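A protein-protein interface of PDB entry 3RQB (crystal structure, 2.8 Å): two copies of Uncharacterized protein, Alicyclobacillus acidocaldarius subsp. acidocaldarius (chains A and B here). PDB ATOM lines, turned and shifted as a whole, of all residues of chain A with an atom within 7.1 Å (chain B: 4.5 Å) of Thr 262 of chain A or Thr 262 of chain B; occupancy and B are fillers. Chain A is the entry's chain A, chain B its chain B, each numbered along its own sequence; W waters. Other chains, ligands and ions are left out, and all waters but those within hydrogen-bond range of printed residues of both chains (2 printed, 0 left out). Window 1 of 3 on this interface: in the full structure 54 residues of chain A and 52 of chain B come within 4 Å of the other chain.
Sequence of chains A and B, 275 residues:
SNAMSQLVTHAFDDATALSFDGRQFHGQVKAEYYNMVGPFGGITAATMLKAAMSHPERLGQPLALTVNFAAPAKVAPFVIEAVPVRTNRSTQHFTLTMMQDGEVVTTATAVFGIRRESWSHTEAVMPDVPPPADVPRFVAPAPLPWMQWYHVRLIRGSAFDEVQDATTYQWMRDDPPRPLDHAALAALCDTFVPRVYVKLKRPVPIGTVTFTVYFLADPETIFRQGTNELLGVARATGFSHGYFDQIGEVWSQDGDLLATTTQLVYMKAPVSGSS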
ATOM      1  N   LEU A  65      25.943  12.685  22.269  1.00  0.00           N
ATOM      2  CA  LEU A  65      26.563  11.973  23.382  1.00  0.00           C
ATOM      3  C   LEU A  65      26.843  12.906  24.549  1.00  0.00           C
ATOM      4  O   LEU A  65      27.346  14.012  24.350  1.00  0.00           O
ATOM      5  CB  LEU A  65      27.863  11.334  22.923  1.00  0.00           C
ATOM      6  CG  LEU A  65      28.748  10.718  23.997  1.00  0.00           C
ATOM      7  CD1 LEU A  65      28.036   9.618  24.778  1.00  0.00           C
ATOM      8  CD2 LEU A  65      29.976  10.178  23.327  1.00  0.00           C
ATOM      9  N   THR A  66      26.513  12.459  25.760  1.00  0.00           N
ATOM     10  CA  THR A  66      26.821  13.220  26.965  1.00  0.00           C
ATOM     11  C   THR A  66      27.593  12.306  27.907  1.00  0.00           C
ATOM     12  O   THR A  66      27.213  11.153  28.124  1.00  0.00           O
ATOM     13  CB  THR A  66      25.554  13.774  27.691  1.00  0.00           C
ATOM     14  OG1 THR A  66      24.813  14.647  26.824  1.00  0.00           O
ATOM     15  CG2 THR A  66      25.960  14.546  28.932  1.00  0.00           C
ATOM     16  N   CYS A 189      36.568  17.939  20.354  1.00  0.00           N
ATOM     17  CA  CYS A 189      35.844  18.936  21.120  1.00  0.00           C
ATOM     18  C   CYS A 189      36.390  19.189  22.534  1.00  0.00           C
ATOM     19  O   CYS A 189      36.015  20.184  23.166  1.00  0.00           O
ATOM     20  CB  CYS A 189      34.382  18.536  21.193  1.00  0.00           C
ATOM     21  SG  CYS A 189      33.600  18.448  19.575  1.00  0.00           S
ATOM     22  N   THR A 208      36.696  18.327  34.249  1.00  0.00           N
ATOM     23  CA  THR A 208      35.427  18.299  33.552  1.00  0.00           C
ATOM     24  C   THR A 208      34.541  17.293  34.227  1.00  0.00           C
ATOM     25  O   THR A 208      34.882  16.119  34.325  1.00  0.00           O
ATOM     26  CB  THR A 208      35.554  17.903  32.084  1.00  0.00           C
ATOM     27  OG1 THR A 208      36.484  18.771  31.431  1.00  0.00           O
ATOM     28  CG2 THR A 208      34.197  18.024  31.397  1.00  0.00           C
ATOM     29  N   THR A 210      31.230  17.192  33.229  1.00  0.00           N
ATOM     30  CA  THR A 210      30.291  16.772  32.223  1.00  0.00           C
ATOM     31  C   THR A 210      30.522  17.464  30.876  1.00  0.00           C
ATOM     32  O   THR A 210      30.946  18.629  30.808  1.00  0.00           O
ATOM     33  CB  THR A 210      28.860  16.956  32.720  1.00  0.00           C
ATOM     34  OG1 THR A 210      27.969  16.183  31.905  1.00  0.00           O
ATOM     35  CG2 THR A 210      28.462  18.420  32.680  1.00  0.00           C
ATOM     36  N   PHE A 211      30.232  16.720  29.811  1.00  0.00           N
ATOM     37  CA  PHE A 211      30.620  17.076  28.448  1.00  0.00           C
ATOM     38  C   PHE A 211      29.553  16.593  27.469  1.00  0.00           C
ATOM     39  O   PHE A 211      28.968  15.513  27.651  1.00  0.00           O
ATOM     40  CB  PHE A 211      31.965  16.420  28.129  1.00  0.00           C
ATOM     41  CG  PHE A 211      32.470  16.683  26.744  1.00  0.00           C
ATOM     42  CD1 PHE A 211      32.304  17.928  26.145  1.00  0.00           C
ATOM     43  CD2 PHE A 211      33.158  15.690  26.050  1.00  0.00           C
ATOM     44  CE1 PHE A 211      32.797  18.174  24.853  1.00  0.00           C
ATOM     45  CE2 PHE A 211      33.656  15.922  24.763  1.00  0.00           C
ATOM     46  CZ  PHE A 211      33.476  17.167  24.166  1.00  0.00           C
ATOM     47  N   THR A 212      29.290  17.394  26.440  1.00  0.00           N
ATOM     48  CA  THR A 212      28.209  17.083  25.503  1.00  0.00           C
ATOM     49  C   THR A 212      28.600  17.416  24.059  1.00  0.00           C
ATOM     50  O   THR A 212      29.137  18.489  23.770  1.00  0.00           O
ATOM     51  CB  THR A 212      26.871  17.804  25.890  1.00  0.00           C
ATOM     52  OG1 THR A 212      26.424  17.373  27.191  1.00  0.00           O
ATOM     53  CG2 THR A 212      25.781  17.513  24.871  1.00  0.00           C
ATOM     54  N   VAL A 213      28.351  16.477  23.153  1.00  0.00           N
ATOM     55  CA  VAL A 213      28.571  16.726  21.733  1.00  0.00           C
ATOM     56  C   VAL A 213      27.333  16.405  20.915  1.00  0.00           C
ATOM     57  O   VAL A 213      26.837  15.283  20.942  1.00  0.00           O
ATOM     58  CB  VAL A 213      29.720  15.885  21.167  1.00  0.00           C
ATOM     59  CG1 VAL A 213      29.769  16.024  19.644  1.00  0.00           C
ATOM     60  CG2 VAL A 213      31.034  16.298  21.791  1.00  0.00           C
ATOM     61  N   TYR A 214      26.823  17.398  20.199  1.00  0.00           N
ATOM     62  CA  TYR A 214      25.784  17.150  19.229  1.00  0.00           C
ATOM     63  C   TYR A 214      26.510  17.056  17.900  1.00  0.00           C
ATOM     64  O   TYR A 214      27.427  17.833  17.646  1.00  0.00           O
ATOM     65  CB  TYR A 214      24.807  18.317  19.207  1.00  0.00           C
ATOM     66  CG  TYR A 214      23.996  18.475  20.465  1.00  0.00           C
ATOM     67  CD1 TYR A 214      23.808  17.410  21.332  1.00  0.00           C
ATOM     68  CD2 TYR A 214      23.405  19.697  20.788  1.00  0.00           C
ATOM     69  CE1 TYR A 214      23.053  17.553  22.491  1.00  0.00           C
ATOM     70  CE2 TYR A 214      22.643  19.853  21.951  1.00  0.00           C
ATOM     71  CZ  TYR A 214      22.469  18.775  22.800  1.00  0.00           C
ATOM     72  OH  TYR A 214      21.714  18.911  23.955  1.00  0.00           O
ATOM     73  N   ASP A 245      31.534  27.264  32.296  1.00  0.00           N
ATOM     74  CA  ASP A 245      31.063  26.397  31.232  1.00  0.00           C
ATOM     75  C   ASP A 245      31.877  26.672  29.990  1.00  0.00           C
ATOM     76  O   ASP A 245      32.582  27.679  29.909  1.00  0.00           O
ATOM     77  CB  ASP A 245      29.597  26.672  30.933  1.00  0.00           C
ATOM     78  CG  ASP A 245      29.397  27.950  30.135  1.00  0.00           C
ATOM     79  OD1 ASP A 245      30.134  28.933  30.378  1.00  0.00           O
ATOM     80  OD2 ASP A 245      28.508  27.966  29.255  1.00  0.00           O
ATOM     81  N   GLN A 246      31.795  25.762  29.030  1.00  0.00           N
ATOM     82  CA  GLN A 246      32.403  25.983  27.723  1.00  0.00           C
ATOM     83  C   GLN A 246      31.409  25.642  26.611  1.00  0.00           C
ATOM     84  O   GLN A 246      30.768  24.585  26.628  1.00  0.00           O
ATOM     85  CB  GLN A 246      33.687  25.161  27.589  1.00  0.00           C
ATOM     86  CG  GLN A 246      34.338  25.225  26.228  1.00  0.00           C
ATOM     87  CD  GLN A 246      35.732  24.627  26.224  1.00  0.00           C
ATOM     88  OE1 GLN A 246      36.677  25.194  26.802  1.00  0.00           O
ATOM     89  NE2 GLN A 246      35.874  23.477  25.565  1.00  0.00           N
ATOM     90  N   ILE A 247      31.257  26.561  25.666  1.00  0.00           N
ATOM     91  CA  ILE A 247      30.441  26.326  24.484  1.00  0.00           C
ATOM     92  C   ILE A 247      31.371  26.314  23.286  1.00  0.00           C
ATOM     93  O   ILE A 247      32.281  27.136  23.186  1.00  0.00           O
ATOM     94  CB  ILE A 247      29.371  27.428  24.288  1.00  0.00           C
ATOM     95  CG1 ILE A 247      28.270  27.305  25.343  1.00  0.00           C
ATOM     96  CG2 ILE A 247      28.781  27.382  22.878  1.00  0.00           C
ATOM     97  CD1 ILE A 247      28.235  28.470  26.318  1.00  0.00           C
ATOM     98  N   GLY A 248      31.132  25.404  22.356  1.00  0.00           N
ATOM     99  CA  GLY A 248      32.029  25.275  21.236  1.00  0.00           C
ATOM    100  C   GLY A 248      31.269  24.944  19.978  1.00  0.00           C
ATOM    101  O   GLY A 248      30.091  24.580  20.029  1.00  0.00           O
ATOM    102  N   THR A 260      28.397  20.772  17.787  1.00  0.00           N
ATOM    103  CA  THR A 260      28.482  21.773  18.849  1.00  0.00           C
ATOM    104  C   THR A 260      28.774  21.016  20.128  1.00  0.00           C
ATOM    105  O   THR A 260      28.505  19.814  20.187  1.00  0.00           O
ATOM    106  CB  THR A 260      27.182  22.581  19.033  1.00  0.00           C
ATOM    107  OG1 THR A 260      26.059  21.689  19.099  1.00  0.00           O
ATOM    108  CG2 THR A 260      26.994  23.560  17.886  1.00  0.00           C
ATOM    109  N   THR A 261      29.336  21.704  21.129  1.00  0.00           N
ATOM    110  CA  THR A 261      29.627  21.113  22.446  1.00  0.00           C
ATOM    111  C   THR A 261      29.333  22.025  23.619  1.00  0.00           C
ATOM    112  O   THR A 261      29.312  23.253  23.507  1.00  0.00           O
ATOM    113  CB  THR A 261      31.114  20.695  22.628  1.00  0.00           C
ATOM    114  OG1 THR A 261      31.973  21.818  22.384  1.00  0.00           O
ATOM    115  CG2 THR A 261      31.473  19.585  21.697  1.00  0.00           C
ATOM    116  N   THR A 262      29.130  21.394  24.765  1.00  0.00           N
ATOM    117  CA  THR A 262      29.115  22.095  26.027  1.00  0.00           C
ATOM    118  C   THR A 262      29.884  21.251  26.998  1.00  0.00           C
ATOM    119  O   THR A 262      29.934  20.024  26.890  1.00  0.00           O
ATOM    120  CB  THR A 262      27.693  22.359  26.574  1.00  0.00           C
ATOM    121  OG1 THR A 262      26.890  21.169  26.486  1.00  0.00           O
ATOM    122  CG2 THR A 262      27.037  23.492  25.795  1.00  0.00           C
ATOM    123  N   GLN A 263      30.493  21.927  27.949  1.00  0.00           N
ATOM    124  CA  GLN A 263      31.290  21.264  28.935  1.00  0.00           C
ATOM    125  C   GLN A 263      30.989  21.987  30.216  1.00  0.00           C
ATOM    126  O   GLN A 263      30.724  23.187  30.200  1.00  0.00           O
ATOM    127  CB  GLN A 263      32.744  21.446  28.572  1.00  0.00           C
ATOM    128  CG  GLN A 263      33.695  20.800  29.514  1.00  0.00           C
ATOM    129  CD  GLN A 263      34.962  20.409  28.800  1.00  0.00           C
ATOM    130  OE1 GLN A 263      34.950  20.191  27.582  1.00  0.00           O
ATOM    131  NE2 GLN A 263      36.067  20.329  29.538  1.00  0.00           N
ATOM    132  N   LEU A 264      31.004  21.275  31.331  1.00  0.00           N
ATOM    133  CA  LEU A 264      30.895  21.971  32.592  1.00  0.00           C
ATOM    134  C   LEU A 264      32.100  21.676  33.441  1.00  0.00           C
ATOM    135  O   LEU A 264      32.453  20.516  33.634  1.00  0.00           O
ATOM    136  CB  LEU A 264      29.633  21.586  33.327  1.00  0.00           C
ATOM    137  CG  LEU A 264      29.463  22.517  34.525  1.00  0.00           C
ATOM    138  CD1 LEU A 264      29.285  23.962  34.052  1.00  0.00           C
ATOM    139  CD2 LEU A 264      28.293  22.065  35.377  1.00  0.00           C
ATOM    140  N   THR B 210      17.153  15.205  23.103  1.00  0.00           N
ATOM    141  CA  THR B 210      17.983  15.412  24.278  1.00  0.00           C
ATOM    142  C   THR B 210      18.061  16.878  24.707  1.00  0.00           C
ATOM    143  O   THR B 210      18.005  17.801  23.883  1.00  0.00           O
ATOM    144  CB  THR B 210      19.400  14.859  24.055  1.00  0.00           C
ATOM    145  OG1 THR B 210      20.179  15.034  25.247  1.00  0.00           O
ATOM    146  CG2 THR B 210      20.058  15.573  22.904  1.00  0.00           C
ATOM    147  N   PHE B 211      18.188  17.071  26.016  1.00  0.00           N
ATOM    148  CA  PHE B 211      18.133  18.382  26.618  1.00  0.00           C
ATOM    149  C   PHE B 211      19.182  18.423  27.729  1.00  0.00           C
ATOM    150  O   PHE B 211      19.205  17.543  28.589  1.00  0.00           O
ATOM    151  CB  PHE B 211      16.711  18.561  27.146  1.00  0.00           C
ATOM    152  CG  PHE B 211      16.495  19.793  27.983  1.00  0.00           C
ATOM    153  CD1 PHE B 211      16.301  21.035  27.393  1.00  0.00           C
ATOM    154  CD2 PHE B 211      16.422  19.697  29.368  1.00  0.00           C
ATOM    155  CE1 PHE B 211      16.075  22.168  28.172  1.00  0.00           C
ATOM    156  CE2 PHE B 211      16.197  20.822  30.148  1.00  0.00           C
ATOM    157  CZ  PHE B 211      16.021  22.059  29.549  1.00  0.00           C
ATOM    158  N   THR B 212      20.062  19.426  27.700  1.00  0.00           N
ATOM    159  CA  THR B 212      21.060  19.589  28.762  1.00  0.00           C
ATOM    160  C   THR B 212      20.924  20.955  29.430  1.00  0.00           C
ATOM    161  O   THR B 212      20.572  21.939  28.778  1.00  0.00           O
ATOM    162  CB  THR B 212      22.520  19.403  28.259  1.00  0.00           C
ATOM    163  OG1 THR B 212      22.746  18.032  27.916  1.00  0.00           O
ATOM    164  CG2 THR B 212      23.506  19.772  29.339  1.00  0.00           C
ATOM    165  N   TYR B 214      23.001  23.447  32.554  1.00  0.00           N
ATOM    166  CA  TYR B 214      24.014  23.681  33.564  1.00  0.00           C
ATOM    167  C   TYR B 214      23.503  24.788  34.474  1.00  0.00           C
ATOM    168  O   TYR B 214      23.061  25.834  33.976  1.00  0.00           O
ATOM    169  CB  TYR B 214      25.306  24.139  32.887  1.00  0.00           C
ATOM    170  CG  TYR B 214      25.928  23.125  31.952  1.00  0.00           C
ATOM    171  CD1 TYR B 214      25.508  21.797  31.948  1.00  0.00           C
ATOM    172  CD2 TYR B 214      26.951  23.492  31.093  1.00  0.00           C
ATOM    173  CE1 TYR B 214      26.092  20.867  31.110  1.00  0.00           C
ATOM    174  CE2 TYR B 214      27.539  22.572  30.248  1.00  0.00           C
ATOM    175  CZ  TYR B 214      27.110  21.262  30.258  1.00  0.00           C
ATOM    176  OH  TYR B 214      27.706  20.352  29.417  1.00  0.00           O
ATOM    177  N   GLN B 246      19.194  23.991  19.942  1.00  0.00           N
ATOM    178  CA  GLN B 246      18.831  25.218  20.607  1.00  0.00           C
ATOM    179  C   GLN B 246      19.878  25.474  21.655  1.00  0.00           C
ATOM    180  O   GLN B 246      20.208  24.585  22.432  1.00  0.00           O
ATOM    181  CB  GLN B 246      17.456  25.078  21.262  1.00  0.00           C
ATOM    182  CG  GLN B 246      16.802  26.401  21.598  1.00  0.00           C
ATOM    183  CD  GLN B 246      15.370  26.239  22.059  1.00  0.00           C
ATOM    184  OE1 GLN B 246      14.450  26.155  21.245  1.00  0.00           O
ATOM    185  NE2 GLN B 246      15.170  26.198  23.375  1.00  0.00           N
ATOM    186  N   THR B 261      21.496  26.261  28.616  1.00  0.00           N
ATOM    187  CA  THR B 261      20.939  25.013  28.113  1.00  0.00           C
ATOM    188  C   THR B 261      21.187  24.790  26.656  1.00  0.00           C
ATOM    189  O   THR B 261      21.310  25.729  25.876  1.00  0.00           O
ATOM    190  CB  THR B 261      19.419  24.956  28.247  1.00  0.00           C
ATOM    191  OG1 THR B 261      18.834  26.007  27.474  1.00  0.00           O
ATOM    192  CG2 THR B 261      19.027  25.112  29.678  1.00  0.00           C
ATOM    193  N   THR B 262      21.208  23.514  26.306  1.00  0.00           N
ATOM    194  CA  THR B 262      21.215  23.087  24.924  1.00  0.00           C
ATOM    195  C   THR B 262      20.128  22.049  24.697  1.00  0.00           C
ATOM    196  O   THR B 262      19.685  21.345  25.618  1.00  0.00           O
ATOM    197  CB  THR B 262      22.568  22.501  24.519  1.00  0.00           C
ATOM    198  OG1 THR B 262      22.789  21.272  25.224  1.00  0.00           O
ATOM    199  CG2 THR B 262      23.677  23.478  24.856  1.00  0.00           C
ATOM    200  N   GLN B 263      19.699  21.973  23.451  1.00  0.00           N
ATOM    201  CA  GLN B 263      18.632  21.080  23.080  1.00  0.00           C
ATOM    202  C   GLN B 263      18.965  20.550  21.706  1.00  0.00           C
ATOM    203  O   GLN B 263      19.354  21.318  20.826  1.00  0.00           O
ATOM    204  CB  GLN B 263      17.331  21.872  23.018  1.00  0.00           C
ATOM    205  CG  GLN B 263      16.074  21.069  23.227  1.00  0.00           C
ATOM    206  CD  GLN B 263      14.926  21.941  23.682  1.00  0.00           C
ATOM    207  OE1 GLN B 263      13.826  21.861  23.148  1.00  0.00           O
ATOM    208  NE2 GLN B 263      15.183  22.786  24.671  1.00  0.00           N
ATOM    209  N   LEU B 264      18.818  19.244  21.517  1.00  0.00           N
ATOM    210  CA  LEU B 264      18.899  18.667  20.183  1.00  0.00           C
ATOM    211  C   LEU B 264      17.508  18.220  19.772  1.00  0.00           C
ATOM    212  O   LEU B 264      16.850  17.456  20.480  1.00  0.00           O
ATOM    213  CB  LEU B 264      19.864  17.488  20.136  1.00  0.00           C
ATOM    214  CG  LEU B 264      20.048  16.966  18.707  1.00  0.00           C
ATOM    215  CD1 LEU B 264      20.515  18.100  17.810  1.00  0.00           C
ATOM    216  CD2 LEU B 264      21.010  15.769  18.618  1.00  0.00           C
HETATM  217  O   HOH W   1      26.943  17.896  29.965  1.00  0.00           O
HETATM  218  O   HOH W   2      21.295  17.133  25.952  1.00  0.00           O
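Among the printed residues, pairs that only touch across the chains: Gln 263 of chain A with Tyr 214 of chain B (3.2 Å), Thr 262 of chain A with Thr 262 of chain B (3.5 Å), Tyr 214 of chain A with Thr 210 of chain B (3.6 Å), Tyr 214 of chain A with Gln 263 of chain B (3.7 Å), Thr 210 of chain A with Tyr 214 of chain B (3.8 Å), Leu 264 of chain A with Tyr 214 of chain B (3.8 Å), Tyr 214 of chain A with Leu 264 of chain B (3.8 Å), Thr 212 of chain A with Thr 212 of chain B (3.8 Å) and Thr 212 of chain A with Tyr 214 of chain B (3.9 Å).
O of Gln 246 of chain A is in hydrogen-bond range of N of Gln 263 of chain A (3.0 Å). The backbone carbonyl oxygen (O) of Thr 210 of chain A lies within hydrogen-bond range of the backbone NH (N) of Leu 264 of chain A (2.7 Å). The backbone NH (N) of Thr 212 of chain A lies within hydrogen-bond range of the backbone carbonyl oxygen (O) of Thr 262 of chain A. The backbone carbonyl oxygen (O) of Thr 260 of chain A sits at hydrogen-bond distance from the backbone NH (N) of Tyr 214 of chain A (2.9 Å). The backbone NH (N) of Thr 212 of chain B is in hydrogen-bond range of the backbone carbonyl oxygen (O) of Thr 262 of chain B (2.9 Å). N of Leu 264 of chain B lies within hydrogen-bond range of O of Thr 210 of chain B (2.9 Å).
The side-chain hydroxyl (OG1) of Thr 262 of chain A is in hydrogen-bond range of the side-chain hydroxyl (OH) of Tyr 214 of chain B, 3.2 Å away. The side-chain hydroxyl (OH) of Tyr 214 of chain A is in hydrogen-bond range of the side-chain hydroxyl (OG1) of Thr 262 of chain B, at 2.9 Å.
Thr 212 of chain B touches its own counterpart, Thr 212 of chain A. Tyr 214 of chain A touches Thr 262 of chain B, and with the chains exchanged Thr 262 of chain A touches Tyr 214 of chain B. Tyr 214 of chain A touches Gln 263 of chain B, and with the chains exchanged Gln 263 of chain A touches Tyr 214 of chain B. Tyr 214 of chain A touches Leu 264 of chain B, and with the chains exchanged Leu 264 of chain A touches Tyr 214 of chain B. 9 positions are printed for both chains.
Printed residues of chain B that touch a printed residue of chain A: Thr 210, Thr 212, Tyr 214, Thr 262, Gln 263 and Leu 264. Among the printed residues, 11 pairs touch across the chains. Among the printed residues, no Asp or Glu carboxylate lies within 4 Å of a Lys or Arg side-chain nitrogen of the other chain.
Phe 211 of chain A touches none of the printed residues of chain B. Of the printed residues of chain B, Thr 212 of chain A touches Thr 212 and Tyr 214. Of the printed residues of chain B, Tyr 214 of chain A touches Thr 210 (3.6 Å), Thr 262 (2.9 Å), Gln 263 (3.7 Å) and Leu 264 (3.8 Å). Of chain B, only Tyr 214 (3.2 Å) and Thr 262 (3.5 Å) come within 4 Å of Thr 262 of chain A. Of the printed residues of chain A, Tyr 214 of chain B touches Thr 210 (3.8 Å), Thr 212 (3.9 Å), Thr 262 (3.2 Å), Gln 263 (3.2 Å) and Leu 264 (3.8 Å). Of chain A, only Tyr 214 (2.9 Å) and Thr 262 (3.5 Å) come within 4 Å of Thr 262 of chain B. The nearest printed residue of chain B that does not touch Thr 262 of chain A is Thr 212 of chain B (4.6 Å). The nearest printed residue of chain A that does not touch Gln 263 of chain B is Thr 260 of chain A (6.9 Å).
Water W2 lies within hydrogen-bond range of OG1 of Thr 210 of chain B (2.5 Å), OG1 of Thr 212 of chain B (2.6 Å), OH of Tyr 214 of chain A (2.7 Å) and N of Phe 211 of chain B (3.1 Å). Water W1 lies within hydrogen-bond range of OH of Tyr 214 of chain B, OG1 of Thr 210 of chain A, OG1 of Thr 212 of chain A and N of Phe 211 of chain A.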
